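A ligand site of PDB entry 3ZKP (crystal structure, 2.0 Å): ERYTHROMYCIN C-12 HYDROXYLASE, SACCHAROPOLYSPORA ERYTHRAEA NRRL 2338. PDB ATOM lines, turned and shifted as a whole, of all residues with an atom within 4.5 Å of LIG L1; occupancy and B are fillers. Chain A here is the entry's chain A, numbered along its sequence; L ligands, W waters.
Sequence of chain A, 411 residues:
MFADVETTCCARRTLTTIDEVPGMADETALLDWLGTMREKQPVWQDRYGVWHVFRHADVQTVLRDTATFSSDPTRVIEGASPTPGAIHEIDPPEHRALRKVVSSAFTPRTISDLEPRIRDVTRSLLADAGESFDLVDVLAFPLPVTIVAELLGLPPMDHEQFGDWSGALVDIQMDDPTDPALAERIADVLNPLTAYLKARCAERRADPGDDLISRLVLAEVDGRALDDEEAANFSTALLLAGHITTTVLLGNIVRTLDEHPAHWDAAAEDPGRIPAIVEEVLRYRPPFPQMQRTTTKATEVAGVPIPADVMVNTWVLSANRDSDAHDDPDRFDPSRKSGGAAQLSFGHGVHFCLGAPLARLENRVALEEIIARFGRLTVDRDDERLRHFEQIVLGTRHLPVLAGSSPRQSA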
ATOM      1  N   ILE A  87     -11.047  20.373  21.185  1.00  0.00           N
ATOM      2  CA  ILE A  87     -12.396  20.387  21.786  1.00  0.00           C
ATOM      3  C   ILE A  87     -12.387  20.157  23.310  1.00  0.00           C
ATOM      4  O   ILE A  87     -13.140  20.807  24.052  1.00  0.00           O
ATOM      5  CB  ILE A  87     -13.380  19.390  21.065  1.00  0.00           C
ATOM      6  CG1 ILE A  87     -14.796  19.517  21.634  1.00  0.00           C
ATOM      7  CG2 ILE A  87     -12.822  17.921  21.094  1.00  0.00           C
ATOM      8  CD1 ILE A  87     -15.832  18.534  20.996  1.00  0.00           C
ATOM      9  N   HIS A  88     -11.507  19.251  23.729  1.00  0.00           N
ATOM     10  CA  HIS A  88     -11.361  18.851  25.134  1.00  0.00           C
ATOM     11  C   HIS A  88     -10.737  19.933  26.017  1.00  0.00           C
ATOM     12  O   HIS A  88     -10.725  19.806  27.258  1.00  0.00           O
ATOM     13  CB  HIS A  88     -10.506  17.572  25.211  1.00  0.00           C
ATOM     14  CG  HIS A  88      -9.155  17.724  24.570  1.00  0.00           C
ATOM     15  ND1 HIS A  88      -8.995  17.968  23.221  1.00  0.00           N
ATOM     16  CD2 HIS A  88      -7.909  17.684  25.106  1.00  0.00           C
ATOM     17  CE1 HIS A  88      -7.703  18.067  22.946  1.00  0.00           C
ATOM     18  NE2 HIS A  88      -7.028  17.900  24.066  1.00  0.00           N
ATOM     19  N   HIS A  95     -17.232  26.037  22.922  1.00  0.00           N
ATOM     20  CA  HIS A  95     -17.352  24.575  22.950  1.00  0.00           C
ATOM     21  C   HIS A  95     -18.579  23.987  22.221  1.00  0.00           C
ATOM     22  O   HIS A  95     -18.445  23.004  21.480  1.00  0.00           O
ATOM     23  CB  HIS A  95     -17.350  24.073  24.401  1.00  0.00           C
ATOM     24  CG  HIS A  95     -17.466  22.590  24.525  1.00  0.00           C
ATOM     25  ND1 HIS A  95     -18.624  21.962  24.953  1.00  0.00           N
ATOM     26  CD2 HIS A  95     -16.585  21.596  24.253  1.00  0.00           C
ATOM     27  CE1 HIS A  95     -18.435  20.660  24.981  1.00  0.00           C
ATOM     28  NE2 HIS A  95     -17.211  20.407  24.538  1.00  0.00           N
ATOM     29  N   ARG A  99     -18.451  21.125  19.251  1.00  0.00           N
ATOM     30  CA  ARG A  99     -19.062  19.795  19.483  1.00  0.00           C
ATOM     31  C   ARG A  99     -20.193  19.510  18.482  1.00  0.00           C
ATOM     32  O   ARG A  99     -20.334  18.385  18.000  1.00  0.00           O
ATOM     33  CB  ARG A  99     -19.565  19.638  20.934  1.00  0.00           C
ATOM     34  CG  ARG A  99     -19.887  18.187  21.334  1.00  0.00           C
ATOM     35  CD  ARG A  99     -20.110  18.044  22.840  1.00  0.00           C
ATOM     36  NE  ARG A  99     -20.826  16.816  23.205  1.00  0.00           N
ATOM     37  CZ  ARG A  99     -20.382  15.882  24.049  1.00  0.00           C
ATOM     38  NH1 ARG A  99     -19.208  16.000  24.647  1.00  0.00           N
ATOM     39  NH2 ARG A  99     -21.142  14.818  24.321  1.00  0.00           N
ATOM     40  N   PHE A 106     -22.357  10.527  16.461  1.00  0.00           N
ATOM     41  CA  PHE A 106     -22.178   9.727  17.665  1.00  0.00           C
ATOM     42  C   PHE A 106     -23.467   9.346  18.378  1.00  0.00           C
ATOM     43  O   PHE A 106     -23.421   8.737  19.444  1.00  0.00           O
ATOM     44  CB  PHE A 106     -21.236  10.447  18.642  1.00  0.00           C
ATOM     45  CG  PHE A 106     -19.815  10.502  18.166  1.00  0.00           C
ATOM     46  CD1 PHE A 106     -18.975   9.405  18.325  1.00  0.00           C
ATOM     47  CD2 PHE A 106     -19.324  11.653  17.543  1.00  0.00           C
ATOM     48  CE1 PHE A 106     -17.646   9.448  17.875  1.00  0.00           C
ATOM     49  CE2 PHE A 106     -17.989  11.731  17.094  1.00  0.00           C
ATOM     50  CZ  PHE A 106     -17.152  10.615  17.263  1.00  0.00           C
ATOM     51  N   VAL A 148     -12.316   3.383  14.765  1.00  0.00           N
ATOM     52  CA  VAL A 148     -12.132   4.816  14.706  1.00  0.00           C
ATOM     53  C   VAL A 148     -11.453   5.253  13.387  1.00  0.00           C
ATOM     54  O   VAL A 148     -11.782   6.302  12.852  1.00  0.00           O
ATOM     55  CB  VAL A 148     -11.420   5.394  15.980  1.00  0.00           C
ATOM     56  CG1 VAL A 148      -9.918   5.040  16.027  1.00  0.00           C
ATOM     57  CG2 VAL A 148     -11.631   6.879  16.070  1.00  0.00           C
ATOM     58  N   LEU A 238      -9.993  13.528  18.022  1.00  0.00           N
ATOM     59  CA  LEU A 238     -10.935  12.456  17.703  1.00  0.00           C
ATOM     60  C   LEU A 238     -10.264  11.086  17.562  1.00  0.00           C
ATOM     61  O   LEU A 238     -10.796  10.081  18.031  1.00  0.00           O
ATOM     62  CB  LEU A 238     -11.769  12.783  16.461  1.00  0.00           C
ATOM     63  CG  LEU A 238     -12.788  13.935  16.609  1.00  0.00           C
ATOM     64  CD1 LEU A 238     -13.152  14.485  15.232  1.00  0.00           C
ATOM     65  CD2 LEU A 238     -14.022  13.478  17.392  1.00  0.00           C
ATOM     66  N   ALA A 241      -8.893   9.967  21.134  1.00  0.00           N
ATOM     67  CA  ALA A 241     -10.063   9.699  21.967  1.00  0.00           C
ATOM     68  C   ALA A 241     -10.700   8.365  21.642  1.00  0.00           C
ATOM     69  O   ALA A 241     -11.247   7.700  22.528  1.00  0.00           O
ATOM     70  CB  ALA A 241     -11.072  10.813  21.817  1.00  0.00           C
ATOM     71  N   GLY A 242     -10.658   8.007  20.362  1.00  0.00           N
ATOM     72  CA  GLY A 242     -11.402   6.873  19.845  1.00  0.00           C
ATOM     73  C   GLY A 242     -10.795   5.503  20.033  1.00  0.00           C
ATOM     74  O   GLY A 242     -11.487   4.513  19.769  1.00  0.00           O
ATOM     75  N   THR A 245      -8.591   4.472  25.295  1.00  0.00           N
ATOM     76  CA  THR A 245      -9.442   4.077  26.416  1.00  0.00           C
ATOM     77  C   THR A 245     -10.295   2.828  26.158  1.00  0.00           C
ATOM     78  O   THR A 245     -10.537   2.016  27.071  1.00  0.00           O
ATOM     79  CB  THR A 245     -10.374   5.222  26.771  1.00  0.00           C
ATOM     80  OG1 THR A 245     -10.875   5.789  25.551  1.00  0.00           O
ATOM     81  CG2 THR A 245      -9.637   6.288  27.573  1.00  0.00           C
ATOM     82  N   THR A 246     -10.756   2.670  24.922  1.00  0.00           N
ATOM     83  CA  THR A 246     -11.538   1.485  24.539  1.00  0.00           C
ATOM     84  C   THR A 246     -10.665   0.227  24.668  1.00  0.00           C
ATOM     85  O   THR A 246     -11.098  -0.783  25.236  1.00  0.00           O
ATOM     86  CB  THR A 246     -12.155   1.660  23.132  1.00  0.00           C
ATOM     87  OG1 THR A 246     -12.870   2.911  23.088  1.00  0.00           O
ATOM     88  CG2 THR A 246     -13.124   0.535  22.825  1.00  0.00           C
ATOM     89  N   LEU A 249     -10.206  -0.377  28.524  1.00  0.00           N
ATOM     90  CA  LEU A 249     -11.447  -0.957  29.082  1.00  0.00           C
ATOM     91  C   LEU A 249     -11.599  -2.448  28.780  1.00  0.00           C
ATOM     92  O   LEU A 249     -11.939  -3.222  29.668  1.00  0.00           O
ATOM     93  CB  LEU A 249     -12.704  -0.225  28.600  1.00  0.00           C
ATOM     94  CG  LEU A 249     -14.009  -0.745  29.250  1.00  0.00           C
ATOM     95  CD1 LEU A 249     -13.996  -0.625  30.791  1.00  0.00           C
ATOM     96  CD2 LEU A 249     -15.254  -0.027  28.696  1.00  0.00           C
ATOM     97  N   LEU A 282     -16.286  -0.096  34.153  1.00  0.00           N
ATOM     98  CA  LEU A 282     -16.035   1.352  34.020  1.00  0.00           C
ATOM     99  C   LEU A 282     -15.937   2.057  35.369  1.00  0.00           C
ATOM    100  O   LEU A 282     -14.990   2.812  35.606  1.00  0.00           O
ATOM    101  CB  LEU A 282     -17.103   2.011  33.133  1.00  0.00           C
ATOM    102  CG  LEU A 282     -16.792   1.927  31.638  1.00  0.00           C
ATOM    103  CD1 LEU A 282     -18.056   2.007  30.810  1.00  0.00           C
ATOM    104  CD2 LEU A 282     -15.790   2.997  31.217  1.00  0.00           C
ATOM    105  N   PRO A 287     -10.633   3.628  32.754  1.00  0.00           N
ATOM    106  CA  PRO A 287      -9.421   3.769  31.928  1.00  0.00           C
ATOM    107  C   PRO A 287      -8.633   5.079  32.154  1.00  0.00           C
ATOM    108  O   PRO A 287      -7.394   5.058  32.199  1.00  0.00           O
ATOM    109  CB  PRO A 287      -9.980   3.684  30.482  1.00  0.00           C
ATOM    110  CG  PRO A 287     -11.208   2.744  30.634  1.00  0.00           C
ATOM    111  CD  PRO A 287     -11.814   3.246  31.952  1.00  0.00           C
ATOM    112  N   PHE A 288      -9.354   6.184  32.313  1.00  0.00           N
ATOM    113  CA  PHE A 288      -8.780   7.503  32.503  1.00  0.00           C
ATOM    114  C   PHE A 288      -9.150   7.891  33.943  1.00  0.00           C
ATOM    115  O   PHE A 288     -10.259   8.340  34.186  1.00  0.00           O
ATOM    116  CB  PHE A 288      -9.405   8.476  31.486  1.00  0.00           C
ATOM    117  CG  PHE A 288      -8.695   9.814  31.335  1.00  0.00           C
ATOM    118  CD1 PHE A 288      -7.311   9.871  31.144  1.00  0.00           C
ATOM    119  CD2 PHE A 288      -9.432  10.998  31.268  1.00  0.00           C
ATOM    120  CE1 PHE A 288      -6.663  11.093  30.945  1.00  0.00           C
ATOM    121  CE2 PHE A 288      -8.792  12.230  31.076  1.00  0.00           C
ATOM    122  CZ  PHE A 288      -7.428  12.279  30.903  1.00  0.00           C
ATOM    123  N   MET A 291      -8.500  13.720  35.535  1.00  0.00           N
ATOM    124  CA  MET A 291      -8.581  14.744  34.495  1.00  0.00           C
ATOM    125  C   MET A 291      -8.250  16.104  35.115  1.00  0.00           C
ATOM    126  O   MET A 291      -8.516  16.312  36.305  1.00  0.00           O
ATOM    127  CB  MET A 291      -9.987  14.778  33.877  1.00  0.00           C
ATOM    128  CG  MET A 291     -10.829  13.520  34.130  1.00  0.00           C
ATOM    129  SD  MET A 291     -12.157  13.375  32.940  1.00  0.00           S
ATOM    130  CE  MET A 291     -13.532  12.977  33.996  1.00  0.00           C
ATOM    131  N   ARG A 293      -8.352  20.446  35.281  1.00  0.00           N
ATOM    132  CA  ARG A 293      -8.999  21.729  35.016  1.00  0.00           C
ATOM    133  C   ARG A 293      -8.032  22.849  35.419  1.00  0.00           C
ATOM    134  O   ARG A 293      -6.986  22.578  36.054  1.00  0.00           O
ATOM    135  CB  ARG A 293     -10.311  21.825  35.788  1.00  0.00           C
ATOM    136  CG  ARG A 293     -11.375  20.793  35.397  1.00  0.00           C
ATOM    137  CD  ARG A 293     -11.700  20.929  33.908  1.00  0.00           C
ATOM    138  NE  ARG A 293     -12.832  20.137  33.465  1.00  0.00           N
ATOM    139  CZ  ARG A 293     -12.749  18.985  32.799  1.00  0.00           C
ATOM    140  NH1 ARG A 293     -11.568  18.422  32.537  1.00  0.00           N
ATOM    141  NH2 ARG A 293     -13.869  18.387  32.397  1.00  0.00           N
ATOM    142  N   SER A 345     -16.967   7.710  34.641  1.00  0.00           N
ATOM    143  CA  SER A 345     -15.756   7.325  33.917  1.00  0.00           C
ATOM    144  C   SER A 345     -15.729   7.870  32.486  1.00  0.00           C
ATOM    145  O   SER A 345     -14.714   7.773  31.803  1.00  0.00           O
ATOM    146  CB  SER A 345     -15.581   5.806  33.937  1.00  0.00           C
ATOM    147  OG  SER A 345     -15.486   5.374  35.280  1.00  0.00           O
ATOM    148  N   PHE A 346     -16.867   8.432  32.045  1.00  0.00           N
ATOM    149  CA  PHE A 346     -17.011   9.118  30.747  1.00  0.00           C
ATOM    150  C   PHE A 346     -17.056  10.629  30.960  1.00  0.00           C
ATOM    151  O   PHE A 346     -17.315  11.427  30.023  1.00  0.00           O
ATOM    152  CB  PHE A 346     -18.294   8.678  30.037  1.00  0.00           C
ATOM    153  CG  PHE A 346     -18.233   7.308  29.385  1.00  0.00           C
ATOM    154  CD1 PHE A 346     -17.211   6.984  28.477  1.00  0.00           C
ATOM    155  CD2 PHE A 346     -19.221   6.353  29.643  1.00  0.00           C
ATOM    156  CE1 PHE A 346     -17.160   5.723  27.866  1.00  0.00           C
ATOM    157  CE2 PHE A 346     -19.183   5.080  29.035  1.00  0.00           C
ATOM    158  CZ  PHE A 346     -18.149   4.763  28.133  1.00  0.00           C
ATOM    159  N   GLY A 347     -16.829  11.039  32.211  1.00  0.00           N
ATOM    160  CA  GLY A 347     -16.828  12.449  32.548  1.00  0.00           C
ATOM    161  C   GLY A 347     -18.197  12.848  33.057  1.00  0.00           C
ATOM    162  O   GLY A 347     -18.982  11.996  33.493  1.00  0.00           O
ATOM    163  N   VAL A 350     -20.586  19.176  30.348  1.00  0.00           N
ATOM    164  CA  VAL A 350     -20.534  19.551  28.919  1.00  0.00           C
ATOM    165  C   VAL A 350     -19.539  18.755  28.065  1.00  0.00           C
ATOM    166  O   VAL A 350     -19.786  18.511  26.884  1.00  0.00           O
ATOM    167  CB  VAL A 350     -20.465  21.118  28.693  1.00  0.00           C
ATOM    168  CG1 VAL A 350     -21.473  21.860  29.607  1.00  0.00           C
ATOM    169  CG2 VAL A 350     -19.054  21.693  28.851  1.00  0.00           C
ATOM    170  N   HIS A 351     -18.442  18.306  28.672  1.00  0.00           N
ATOM    171  CA  HIS A 351     -17.438  17.489  27.964  1.00  0.00           C
ATOM    172  C   HIS A 351     -17.705  15.975  28.037  1.00  0.00           C
ATOM    173  O   HIS A 351     -16.868  15.194  27.572  1.00  0.00           O
ATOM    174  CB  HIS A 351     -16.027  17.812  28.471  1.00  0.00           C
ATOM    175  CG  HIS A 351     -15.575  19.203  28.166  1.00  0.00           C
ATOM    176  ND1 HIS A 351     -14.970  19.548  26.978  1.00  0.00           N
ATOM    177  CD2 HIS A 351     -15.644  20.341  28.898  1.00  0.00           C
ATOM    178  CE1 HIS A 351     -14.659  20.833  27.000  1.00  0.00           C
ATOM    179  NE2 HIS A 351     -15.075  21.338  28.153  1.00  0.00           N
ATOM    180  N   PHE A 352     -18.839  15.556  28.603  1.00  0.00           N
ATOM    181  CA  PHE A 352     -19.169  14.132  28.727  1.00  0.00           C
ATOM    182  C   PHE A 352     -18.912  13.404  27.408  1.00  0.00           C
ATOM    183  O   PHE A 352     -19.348  13.849  26.336  1.00  0.00           O
ATOM    184  CB  PHE A 352     -20.611  13.931  29.219  1.00  0.00           C
ATOM    185  CG  PHE A 352     -20.986  12.470  29.476  1.00  0.00           C
ATOM    186  CD1 PHE A 352     -21.498  11.667  28.452  1.00  0.00           C
ATOM    187  CD2 PHE A 352     -20.853  11.922  30.761  1.00  0.00           C
ATOM    188  CE1 PHE A 352     -21.863  10.343  28.708  1.00  0.00           C
ATOM    189  CE2 PHE A 352     -21.218  10.597  31.017  1.00  0.00           C
ATOM    190  CZ  PHE A 352     -21.718   9.807  29.990  1.00  0.00           C
ATOM    191  N   CYS A 353     -18.206  12.271  27.500  1.00  0.00           N
ATOM    192  CA  CYS A 353     -17.690  11.557  26.346  1.00  0.00           C
ATOM    193  C   CYS A 353     -18.656  11.451  25.170  1.00  0.00           C
ATOM    194  O   CYS A 353     -19.703  10.806  25.243  1.00  0.00           O
ATOM    195  CB  CYS A 353     -17.274  10.142  26.756  1.00  0.00           C
ATOM    196  SG  CYS A 353     -16.630   9.175  25.412  1.00  0.00           S
ATOM    197  N   LEU A 354     -18.252  12.033  24.060  1.00  0.00           N
ATOM    198  CA  LEU A 354     -19.030  11.986  22.833  1.00  0.00           C
ATOM    199  C   LEU A 354     -19.111  10.538  22.330  1.00  0.00           C
ATOM    200  O   LEU A 354     -20.087  10.152  21.680  1.00  0.00           O
ATOM    201  CB  LEU A 354     -18.321  12.852  21.813  1.00  0.00           C
ATOM    202  CG  LEU A 354     -18.998  13.563  20.654  1.00  0.00           C
ATOM    203  CD1 LEU A 354     -20.440  13.995  20.949  1.00  0.00           C
ATOM    204  CD2 LEU A 354     -18.102  14.739  20.343  1.00  0.00           C
ATOM    205  N   GLY A 355     -18.081   9.749  22.629  1.00  0.00           N
ATOM    206  CA  GLY A 355     -17.968   8.363  22.139  1.00  0.00           C
ATOM    207  C   GLY A 355     -18.608   7.297  23.017  1.00  0.00           C
ATOM    208  O   GLY A 355     -18.459   6.101  22.739  1.00  0.00           O
ATOM    209  N   LEU A 358     -20.592   4.467  21.453  1.00  0.00           N
ATOM    210  CA  LEU A 358     -19.664   3.657  20.673  1.00  0.00           C
ATOM    211  C   LEU A 358     -18.769   2.791  21.567  1.00  0.00           C
ATOM    212  O   LEU A 358     -18.629   1.587  21.319  1.00  0.00           O
ATOM    213  CB  LEU A 358     -18.815   4.532  19.737  1.00  0.00           C
ATOM    214  CG  LEU A 358     -17.781   3.800  18.869  1.00  0.00           C
ATOM    215  CD1 LEU A 358     -18.389   2.711  17.957  1.00  0.00           C
ATOM    216  CD2 LEU A 358     -16.957   4.779  18.057  1.00  0.00           C
ATOM    217  N   ALA A 359     -18.177   3.382  22.600  1.00  0.00           N
ATOM    218  CA  ALA A 359     -17.387   2.598  23.550  1.00  0.00           C
ATOM    219  C   ALA A 359     -18.186   1.429  24.152  1.00  0.00           C
ATOM    220  O   ALA A 359     -17.666   0.303  24.305  1.00  0.00           O
ATOM    221  CB  ALA A 359     -16.837   3.474  24.652  1.00  0.00           C
HETATM  222  C1  LIG L   1     -14.336  12.950  26.137  1.00  0.00           C
HETATM  223  C2  LIG L   1     -13.630   8.718  28.422  1.00  0.00           C
HETATM  224  C3  LIG L   1     -14.157   6.246  24.296  1.00  0.00           C
HETATM  225  C4  LIG L   1     -14.561  10.481  21.850  1.00  0.00           C
HETATM  226  C5  LIG L   1     -14.112  12.023  27.140  1.00  0.00           C
HETATM  227  C6  LIG L   1     -13.976  12.279  28.561  1.00  0.00           C
HETATM  228  C7  LIG L   1     -13.789  11.106  29.188  1.00  0.00           C
HETATM  229  C8  LIG L   1     -13.798  10.064  28.191  1.00  0.00           C
HETATM  230  C9  LIG L   1     -13.584  10.886  30.725  1.00  0.00           C
HETATM  231  C10 LIG L   1     -14.052  13.673  29.219  1.00  0.00           C
HETATM  232  C11 LIG L   1     -12.687  14.294  29.482  1.00  0.00           C
HETATM  233  C12 LIG L   1     -12.826  15.644  30.204  1.00  0.00           C
HETATM  234  O1  LIG L   1     -13.895  15.960  30.808  1.00  0.00           O
HETATM  235  O2  LIG L   1     -11.835  16.416  30.197  1.00  0.00           O
HETATM  236  C13 LIG L   1     -13.713   7.662  27.535  1.00  0.00           C
HETATM  237  C14 LIG L   1     -13.598   6.252  27.854  1.00  0.00           C
HETATM  238  C15 LIG L   1     -13.748   5.554  26.718  1.00  0.00           C
HETATM  239  C16 LIG L   1     -13.955   6.508  25.637  1.00  0.00           C
HETATM  240  C17 LIG L   1     -13.345   5.742  29.294  1.00  0.00           C
HETATM  241  C18 LIG L   1     -13.689   4.016  26.487  1.00  0.00           C
HETATM  242  C19 LIG L   1     -14.272   3.101  27.279  1.00  0.00           C
HETATM  243  C20 LIG L   1     -14.332   7.172  23.281  1.00  0.00           C
HETATM  244  C21 LIG L   1     -14.537   6.850  21.885  1.00  0.00           C
HETATM  245  C22 LIG L   1     -14.647   8.018  21.207  1.00  0.00           C
HETATM  246  C23 LIG L   1     -14.513   9.113  22.147  1.00  0.00           C
HETATM  247  C24 LIG L   1     -14.631   5.414  21.316  1.00  0.00           C
HETATM  248  C25 LIG L   1     -14.871   8.164  19.691  1.00  0.00           C
HETATM  249  C26 LIG L   1     -14.096   9.020  19.010  1.00  0.00           C
HETATM  250  C27 LIG L   1     -14.508  11.530  22.755  1.00  0.00           C
HETATM  251  C28 LIG L   1     -14.504  12.939  22.402  1.00  0.00           C
HETATM  252  C29 LIG L   1     -14.423  13.679  23.726  1.00  0.00           C
HETATM  253  C30 LIG L   1     -14.409  12.680  24.769  1.00  0.00           C
HETATM  254  C31 LIG L   1     -14.506  13.556  20.984  1.00  0.00           C
HETATM  255  C32 LIG L   1     -14.376  15.192  23.942  1.00  0.00           C
HETATM  256  C33 LIG L   1     -15.789  15.640  24.311  1.00  0.00           C
HETATM  257  C34 LIG L   1     -15.793  17.114  24.597  1.00  0.00           C
HETATM  258  O3  LIG L   1     -14.735  17.631  25.024  1.00  0.00           O
HETATM  259  O4  LIG L   1     -16.868  17.754  24.411  1.00  0.00           O
HETATM  260  N1  LIG L   1     -14.004  10.644  26.951  1.00  0.00           N
HETATM  261  N2  LIG L   1     -13.901   7.769  26.165  1.00  0.00           N
HETATM  262  N3  LIG L   1     -14.302   8.562  23.396  1.00  0.00           N
HETATM  263  N4  LIG L   1     -14.459  11.432  24.153  1.00  0.00           N
HETATM  264 FE1  LIG L   1     -14.351   9.572  25.232  1.00  0.00          FE
HETATM  265  C1  LG2 L   2      -7.423  13.474  24.059  1.00  0.00           C
HETATM  266  N1  LG2 L   2      -2.144  14.737  32.304  1.00  0.00           N
HETATM  267  O1  LG2 L   2      -7.213  12.333  23.686  1.00  0.00           O
HETATM  268  C2  LG2 L   2      -6.433  14.623  23.965  1.00  0.00           C
HETATM  269  O2  LG2 L   2      -8.690  13.841  24.633  1.00  0.00           O
HETATM  270  C3  LG2 L   2      -5.160  14.385  24.816  1.00  0.00           C
HETATM  271  O3  LG2 L   2      -4.508  15.661  24.940  1.00  0.00           O
HETATM  272  C4  LG2 L   2      -5.491  13.802  26.199  1.00  0.00           C
HETATM  273  O4  LG2 L   2      -2.554  16.204  26.088  1.00  0.00           O
HETATM  274  C5  LG2 L   2      -4.341  12.925  26.758  1.00  0.00           C
HETATM  275  O5  LG2 L   2      -4.050  18.386  23.575  1.00  0.00           O
HETATM  276  C6  LG2 L   2      -4.484  11.426  26.463  1.00  0.00           C
HETATM  277  O6  LG2 L   2      -2.530  19.801  25.463  1.00  0.00           O
HETATM  278  C7  LG2 L   2      -5.563  10.843  27.393  1.00  0.00           C
HETATM  279  O7  LG2 L   2      -4.245  13.049  28.182  1.00  0.00           O
HETATM  280  C8  LG2 L   2      -6.405   9.654  26.895  1.00  0.00           C
HETATM  281  O8  LG2 L   2      -4.562  14.323  30.718  1.00  0.00           O
HETATM  282  C9  LG2 L   2      -7.690   9.507  27.715  1.00  0.00           C
HETATM  283  O9  LG2 L   2      -1.933  13.370  28.305  1.00  0.00           O
HETATM  284  C10 LG2 L   2      -8.846  10.503  27.599  1.00  0.00           C
HETATM  285  O10 LG2 L   2      -4.820  11.234  25.083  1.00  0.00           O
HETATM  286  C11 LG2 L   2      -8.922  11.095  26.186  1.00  0.00           C
HETATM  287  O11 LG2 L   2      -7.806   8.593  28.508  1.00  0.00           O
HETATM  288  C12 LG2 L   2      -9.877  12.290  26.046  1.00  0.00           C
HETATM  289  O12 LG2 L   2      -9.270  10.043  25.283  1.00  0.00           O
HETATM  290  C13 LG2 L   2      -9.763  12.924  24.657  1.00  0.00           C
HETATM  291  C14 LG2 L   2      -3.072  15.670  24.851  1.00  0.00           C
HETATM  292  C15 LG2 L   2      -2.572  16.474  23.632  1.00  0.00           C
HETATM  293  C16 LG2 L   2      -2.689  18.009  23.798  1.00  0.00           C
HETATM  294  C17 LG2 L   2      -2.265  18.420  25.215  1.00  0.00           C
HETATM  295  C18 LG2 L   2      -2.916  17.559  26.315  1.00  0.00           C
HETATM  296  C19 LG2 L   2      -1.803  18.673  22.711  1.00  0.00           C
HETATM  297  C20 LG2 L   2      -4.437  19.493  22.734  1.00  0.00           C
HETATM  298  C21 LG2 L   2      -2.466  17.949  27.718  1.00  0.00           C
HETATM  299  C22 LG2 L   2      -3.201  13.883  28.713  1.00  0.00           C
HETATM  300  C23 LG2 L   2      -3.257  13.893  30.235  1.00  0.00           C
HETATM  301  C24 LG2 L   2      -2.106  14.734  30.812  1.00  0.00           C
HETATM  302  C25 LG2 L   2      -0.755  14.264  30.215  1.00  0.00           C
HETATM  303  C26 LG2 L   2      -0.830  14.199  28.687  1.00  0.00           C
HETATM  304  C27 LG2 L   2       0.447  13.587  28.084  1.00  0.00           C
HETATM  305  C28 LG2 L   2      -1.833  13.436  32.967  1.00  0.00           C
HETATM  306  C29 LG2 L   2      -1.233  15.762  32.835  1.00  0.00           C
HETATM  307  C30 LG2 L   2      -6.175  14.976  22.488  1.00  0.00           C
HETATM  308  C31 LG2 L   2      -5.953  14.905  27.165  1.00  0.00           C
HETATM  309  C32 LG2 L   2      -3.132  10.719  26.694  1.00  0.00           C
HETATM  310  C33 LG2 L   2      -5.577   8.361  26.912  1.00  0.00           C
HETATM  311  C34 LG2 L   2     -10.192   9.902  28.028  1.00  0.00           C
HETATM  312  C35 LG2 L   2      -9.689  13.296  27.196  1.00  0.00           C
HETATM  313  C36 LG2 L   2     -10.977  13.790  24.322  1.00  0.00           C
HETATM  314  C37 LG2 L   2     -10.876  14.289  22.897  1.00  0.00           C
HETATM  315  O   HOH W   1      -9.242  15.953  29.640  1.00  0.00           O
HETATM  316  O   HOH W   2     -16.459  15.730  31.532  1.00  0.00           O
HETATM  317  O   HOH W   3     -11.200   5.031  23.270  1.00  0.00           O
HETATM  318  O   HOH W   4     -11.672   9.177  24.850  1.00  0.00           O
HETATM  319  O   HOH W   5     -12.543  18.862  29.005  1.00  0.00           O
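The guanidinium group (NH2) of Arg 293 is in salt-bridge range of an oxygen (O1) of LIG L1 (2.9 Å).
An oxygen (O3) of LIG L1 is in hydrogen-bond range of a ring nitrogen (ND1) of His 351.
A ring nitrogen (NE2) of His 95 is in hydrogen-bond range of an oxygen (O4) of LIG L1 (2.7 Å).
NE2 of His 88 is in hydrogen-bond range of O5 of LG2 L2 (3.1 Å).
NH1 of Arg 99 is in salt-bridge range of O4 of LIG L1, 2.9 Å away.
SG of Cys 353 is bound to FE1 of LIG L1 (2.3 Å).
Water W4 bridges O12 of LG2 L2 (2.6 Å) and O of Ala 241 (2.8 Å).
Water W5 lies within hydrogen-bond range of the backbone carbonyl oxygen (O) of His 88 (2.7 Å), an oxygen (O2) of LIG L1 (2.8 Å) and a ring nitrogen (ND1) of His 351 (3.2 Å).
Water W3 lies within hydrogen-bond range of OG1 of Thr 245 (2.4 Å), OG1 of Thr 246 (2.7 Å) and O of Ala 241 (2.8 Å).
A nitrogen (N3) of LIG L1 lies close to the backbone carbonyl oxygen of Ala 241 (3.3 Å).
SD of Met 291 lies close to O1 of LIG L1, 3.8 Å away.
Ile 87 touches LIG L1 (CD1 to O4, 3.7 Å).
His 88 touches LIG L1.
Phe 106 touches LIG L1 (CE1 to C25, 3.6 Å).
Leu 238 touches LIG L1 (O to C26, 3.6 Å).
CA of Gly 242 touches C26 of LIG L1, at 3.5 Å.
Thr 245 touches LIG L1 (OG1 to C15, 3.1 Å).
OG1 of Thr 246 touches C24 of LIG L1, 3.5 Å away.
CD2 of Leu 249 touches C19 of LIG L1, at 3.6 Å.
Pro 287 touches LIG L1 (CG to C17, 3.9 Å).
Ser 345 touches LIG L1 (O to C9, 3.5 Å).
Phe 346 touches LIG L1.
Gly 347 touches LIG L1.
O of Val 350 touches O4 of LIG L1, at 3.9 Å.
Leu 354 touches LIG L1 (CD2 to C31, 3.8 Å).
Gly 355 touches LIG L1.
CB of Ala 359 touches C18 of LIG L1, 3.7 Å away.
Hydrophobic or aromatic side chains within 4 Å of LIG L1: Ile 87, His 95, Phe 106, Leu 238, Ala 241, Leu 249, Pro 287, Met 291, Phe 346, His 351, Leu 354 and Ala 359.
Of the 28 residues printed, 23 come within 4 Å of LIG L1.
The side-chain hydroxyl (OG) of Ser 345 is in hydrogen-bond range of the backbone carbonyl oxygen (O) of Leu 282 (2.6 Å).
The backbone carbonyl oxygen (O) of Val 350 lies within hydrogen-bond range of the guanidinium group (NH1) of Arg 99, 3.4 Å away.
NH1 of Arg 99 is in hydrogen-bond range of O of Phe 352, at 2.7 Å.
The side-chain sulfur (SG) of Cys 353 lies close to the backbone NH (N) of Gly 355, 3.2 Å away.
The backbone carbonyl oxygen (O) of Phe 346 is in hydrogen-bond range of the backbone NH (N) of Cys 353, at 2.8 Å.
A ring nitrogen (NE2) of His 95 sits at hydrogen-bond distance from a ring nitrogen (ND1) of His 351, at 3.4 Å.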
